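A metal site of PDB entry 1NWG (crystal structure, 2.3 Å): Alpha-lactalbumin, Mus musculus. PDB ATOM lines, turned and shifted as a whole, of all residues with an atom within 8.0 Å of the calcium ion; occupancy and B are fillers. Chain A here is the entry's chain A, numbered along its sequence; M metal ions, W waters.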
ATOM      1  N   THR A  38      21.969 -32.599 -22.650  1.00  0.00           N
ATOM      2  CA  THR A  38      21.340 -31.710 -23.632  1.00  0.00           C
ATOM      3  C   THR A  38      19.886 -32.082 -23.938  1.00  0.00           C
ATOM      4  O   THR A  38      19.139 -31.237 -24.478  1.00  0.00           O
ATOM      5  CB  THR A  38      22.101 -31.700 -24.980  1.00  0.00           C
ATOM      6  OG1 THR A  38      22.161 -33.034 -25.502  1.00  0.00           O
ATOM      7  CG2 THR A  38      23.510 -31.146 -24.797  1.00  0.00           C
ATOM      8  N   ILE A  75      11.739 -19.081 -30.049  1.00  0.00           N
ATOM      9  CA  ILE A  75      12.307 -20.327 -30.513  1.00  0.00           C
ATOM     10  C   ILE A  75      11.368 -21.449 -30.164  1.00  0.00           C
ATOM     11  O   ILE A  75      10.627 -21.358 -29.188  1.00  0.00           O
ATOM     12  CB  ILE A  75      13.638 -20.549 -29.749  1.00  0.00           C
ATOM     13  CG1 ILE A  75      14.414 -21.735 -30.309  1.00  0.00           C
ATOM     14  CG2 ILE A  75      13.310 -20.832 -28.276  1.00  0.00           C
ATOM     15  CD1 ILE A  75      15.644 -22.114 -29.440  1.00  0.00           C
ATOM     16  N   SER A  76      11.405 -22.513 -30.956  1.00  0.00           N
ATOM     17  CA  SER A  76      10.594 -23.688 -30.667  1.00  0.00           C
ATOM     18  C   SER A  76      11.279 -24.481 -29.530  1.00  0.00           C
ATOM     19  O   SER A  76      12.498 -24.695 -29.556  1.00  0.00           O
ATOM     20  CB  SER A  76      10.493 -24.561 -31.920  1.00  0.00           C
ATOM     21  OG  SER A  76       9.861 -25.774 -31.590  1.00  0.00           O
ATOM     22  N   CYS A  77      10.520 -24.920 -28.531  1.00  0.00           N
ATOM     23  CA  CYS A  77      11.145 -25.650 -27.436  1.00  0.00           C
ATOM     24  C   CYS A  77      11.978 -26.861 -27.853  1.00  0.00           C
ATOM     25  O   CYS A  77      12.936 -27.226 -27.154  1.00  0.00           O
ATOM     26  CB  CYS A  77      10.114 -26.119 -26.427  1.00  0.00           C
ATOM     27  SG  CYS A  77       9.196 -24.802 -25.570  1.00  0.00           S
ATOM     28  N   ASP A  78      11.633 -27.484 -28.969  1.00  0.00           N
ATOM     29  CA  ASP A  78      12.369 -28.659 -29.388  1.00  0.00           C
ATOM     30  C   ASP A  78      13.783 -28.267 -29.810  1.00  0.00           C
ATOM     31  O   ASP A  78      14.656 -29.123 -29.953  1.00  0.00           O
ATOM     32  CB  ASP A  78      11.623 -29.398 -30.510  1.00  0.00           C
ATOM     33  CG  ASP A  78      10.290 -30.036 -30.049  1.00  0.00           C
ATOM     34  OD1 ASP A  78      10.167 -30.356 -28.840  1.00  0.00           O
ATOM     35  OD2 ASP A  78       9.374 -30.255 -30.892  1.00  0.00           O
ATOM     36  N   LYS A  79      14.011 -26.962 -30.000  1.00  0.00           N
ATOM     37  CA  LYS A  79      15.320 -26.469 -30.393  1.00  0.00           C
ATOM     38  C   LYS A  79      16.310 -26.528 -29.228  1.00  0.00           C
ATOM     39  O   LYS A  79      17.517 -26.473 -29.416  1.00  0.00           O
ATOM     40  CB  LYS A  79      15.218 -25.014 -30.889  1.00  0.00           C
ATOM     41  CG  LYS A  79      14.866 -24.840 -32.359  1.00  0.00           C
ATOM     42  CD  LYS A  79      15.997 -25.311 -33.223  1.00  0.00           C
ATOM     43  CE  LYS A  79      15.702 -25.041 -34.690  1.00  0.00           C
ATOM     44  NZ  LYS A  79      16.880 -25.328 -35.573  1.00  0.00           N
ATOM     45  N   LEU A  80      15.779 -26.628 -28.011  1.00  0.00           N
ATOM     46  CA  LEU A  80      16.633 -26.682 -26.848  1.00  0.00           C
ATOM     47  C   LEU A  80      16.955 -28.117 -26.480  1.00  0.00           C
ATOM     48  O   LEU A  80      17.336 -28.385 -25.343  1.00  0.00           O
ATOM     49  CB  LEU A  80      15.930 -25.977 -25.698  1.00  0.00           C
ATOM     50  CG  LEU A  80      15.576 -24.524 -26.003  1.00  0.00           C
ATOM     51  CD1 LEU A  80      14.610 -24.004 -24.943  1.00  0.00           C
ATOM     52  CD2 LEU A  80      16.859 -23.667 -26.081  1.00  0.00           C
ATOM     53  N   LEU A  81      16.832 -29.024 -27.443  1.00  0.00           N
ATOM     54  CA  LEU A  81      17.074 -30.448 -27.220  1.00  0.00           C
ATOM     55  C   LEU A  81      18.060 -31.079 -28.175  1.00  0.00           C
ATOM     56  O   LEU A  81      18.081 -32.305 -28.340  1.00  0.00           O
ATOM     57  CB  LEU A  81      15.751 -31.222 -27.301  1.00  0.00           C
ATOM     58  CG  LEU A  81      14.675 -30.985 -26.239  1.00  0.00           C
ATOM     59  CD1 LEU A  81      13.432 -31.846 -26.596  1.00  0.00           C
ATOM     60  CD2 LEU A  81      15.193 -31.354 -24.850  1.00  0.00           C
ATOM     61  N   ASP A  82      18.880 -30.275 -28.832  1.00  0.00           N
ATOM     62  CA  ASP A  82      19.877 -30.835 -29.726  1.00  0.00           C
ATOM     63  C   ASP A  82      21.255 -30.517 -29.143  1.00  0.00           C
ATOM     64  O   ASP A  82      21.364 -30.110 -27.984  1.00  0.00           O
ATOM     65  CB  ASP A  82      19.747 -30.245 -31.118  1.00  0.00           C
ATOM     66  CG  ASP A  82      19.540 -28.767 -31.094  1.00  0.00           C
ATOM     67  OD1 ASP A  82      20.312 -28.068 -30.391  1.00  0.00           O
ATOM     68  OD2 ASP A  82      18.591 -28.296 -31.780  1.00  0.00           O
ATOM     69  N   ASP A  83      22.308 -30.720 -29.920  1.00  0.00           N
ATOM     70  CA  ASP A  83      23.628 -30.465 -29.373  1.00  0.00           C
ATOM     71  C   ASP A  83      24.174 -29.091 -29.755  1.00  0.00           C
ATOM     72  O   ASP A  83      25.334 -28.769 -29.424  1.00  0.00           O
ATOM     73  CB  ASP A  83      24.604 -31.570 -29.793  1.00  0.00           C
ATOM     74  CG  ASP A  83      24.371 -32.858 -29.035  1.00  0.00           C
ATOM     75  OD1 ASP A  83      23.613 -32.864 -28.031  1.00  0.00           O
ATOM     76  OD2 ASP A  83      24.971 -33.879 -29.437  1.00  0.00           O
ATOM     77  N   GLU A  84      23.346 -28.288 -30.431  1.00  0.00           N
ATOM     78  CA  GLU A  84      23.730 -26.946 -30.840  1.00  0.00           C
ATOM     79  C   GLU A  84      23.225 -26.029 -29.748  1.00  0.00           C
ATOM     80  O   GLU A  84      22.040 -25.703 -29.651  1.00  0.00           O
ATOM     81  CB  GLU A  84      23.144 -26.604 -32.192  1.00  0.00           C
ATOM     82  CG  GLU A  84      23.771 -27.433 -33.297  1.00  0.00           C
ATOM     83  CD  GLU A  84      22.916 -27.547 -34.546  1.00  0.00           C
ATOM     84  OE1 GLU A  84      22.680 -28.692 -34.979  1.00  0.00           O
ATOM     85  OE2 GLU A  84      22.497 -26.531 -35.098  1.00  0.00           O
ATOM     86  N   LEU A  85      24.179 -25.613 -28.924  1.00  0.00           N
ATOM     87  CA  LEU A  85      23.935 -24.791 -27.769  1.00  0.00           C
ATOM     88  C   LEU A  85      23.774 -23.288 -27.930  1.00  0.00           C
ATOM     89  O   LEU A  85      23.390 -22.609 -26.975  1.00  0.00           O
ATOM     90  CB  LEU A  85      25.063 -25.058 -26.765  1.00  0.00           C
ATOM     91  CG  LEU A  85      25.035 -26.311 -25.910  1.00  0.00           C
ATOM     92  CD1 LEU A  85      24.303 -27.432 -26.607  1.00  0.00           C
ATOM     93  CD2 LEU A  85      26.444 -26.696 -25.590  1.00  0.00           C
ATOM     94  N   ASP A  86      24.044 -22.749 -29.122  1.00  0.00           N
ATOM     95  CA  ASP A  86      23.929 -21.293 -29.296  1.00  0.00           C
ATOM     96  C   ASP A  86      22.547 -20.723 -28.961  1.00  0.00           C
ATOM     97  O   ASP A  86      22.464 -19.770 -28.196  1.00  0.00           O
ATOM     98  CB  ASP A  86      24.317 -20.856 -30.713  1.00  0.00           C
ATOM     99  CG  ASP A  86      25.710 -21.354 -31.113  1.00  0.00           C
ATOM    100  OD1 ASP A  86      25.851 -22.593 -31.230  1.00  0.00           O
ATOM    101  OD2 ASP A  86      26.644 -20.526 -31.317  1.00  0.00           O
ATOM    102  N   ASP A  87      21.477 -21.292 -29.501  1.00  0.00           N
ATOM    103  CA  ASP A  87      20.176 -20.742 -29.193  1.00  0.00           C
ATOM    104  C   ASP A  87      19.862 -20.887 -27.712  1.00  0.00           C
ATOM    105  O   ASP A  87      19.342 -19.950 -27.095  1.00  0.00           O
ATOM    106  CB  ASP A  87      19.054 -21.339 -30.092  1.00  0.00           C
ATOM    107  CG  ASP A  87      19.114 -22.864 -30.216  1.00  0.00           C
ATOM    108  OD1 ASP A  87      19.643 -23.553 -29.316  1.00  0.00           O
ATOM    109  OD2 ASP A  87      18.597 -23.363 -31.234  1.00  0.00           O
ATOM    110  N   ASP A  88      20.177 -22.047 -27.129  1.00  0.00           N
ATOM    111  CA  ASP A  88      19.954 -22.295 -25.694  1.00  0.00           C
ATOM    112  C   ASP A  88      20.612 -21.178 -24.863  1.00  0.00           C
ATOM    113  O   ASP A  88      20.020 -20.646 -23.921  1.00  0.00           O
ATOM    114  CB  ASP A  88      20.629 -23.608 -25.270  1.00  0.00           C
ATOM    115  CG  ASP A  88      20.181 -24.799 -26.086  1.00  0.00           C
ATOM    116  OD1 ASP A  88      19.598 -25.727 -25.497  1.00  0.00           O
ATOM    117  OD2 ASP A  88      20.430 -24.822 -27.301  1.00  0.00           O
ATOM    118  N   ILE A  89      21.847 -20.865 -25.227  1.00  0.00           N
ATOM    119  CA  ILE A  89      22.627 -19.836 -24.538  1.00  0.00           C
ATOM    120  C   ILE A  89      21.963 -18.480 -24.782  1.00  0.00           C
ATOM    121  O   ILE A  89      21.772 -17.679 -23.856  1.00  0.00           O
ATOM    122  CB  ILE A  89      24.099 -19.867 -25.072  1.00  0.00           C
ATOM    123  CG1 ILE A  89      24.718 -21.240 -24.749  1.00  0.00           C
ATOM    124  CG2 ILE A  89      24.926 -18.746 -24.446  1.00  0.00           C
ATOM    125  CD1 ILE A  89      26.019 -21.554 -25.484  1.00  0.00           C
HETATM  126 CA    CA M   1      19.897 -25.904 -29.249  1.00  0.00          CA
HETATM  127  O   HOH W   1      19.558 -25.685 -31.753  1.00  0.00           O
HETATM  128  O   HOH W   2      19.544 -27.742 -27.602  1.00  0.00           O
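Five residues have an atom within 4 Å of the calcium ion: Lys 79, Asp 82, Glu 84, Asp 87 and Asp 88. The nearest printed residue that does not touch the calcium ion is Leu 80 (4.1 Å).
O of Glu 84 is bound to the calcium ion (2.2 Å). The calcium ion is bound by the side-chain carboxylate (OD2) of Asp 88, 2.3 Å away. The calcium ion is bound by OD1 of Asp 87 (2.4 Å). The calcium ion is bound by the backbone carbonyl oxygen (O) of Lys 79 (2.5 Å). The side-chain carboxylate (OD1) of Asp 82 binds the calcium ion, at 2.5 Å. The calcium ion is bound by water W2. Water W1 binds the calcium ion, 2.5 Å away. The calcium ion has seven donor atoms within binding distance.
Water W1 lies within hydrogen-bond range of OD2 of Asp 87 (2.6 Å) and OD2 of Asp 82 (2.8 Å). Water W2 lies within hydrogen-bond range of N of Asp 82 (2.9 Å), OD1 of Asp 88 (2.9 Å), N of Leu 81 (3.0 Å) and O of Leu 80 (3.2 Å).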
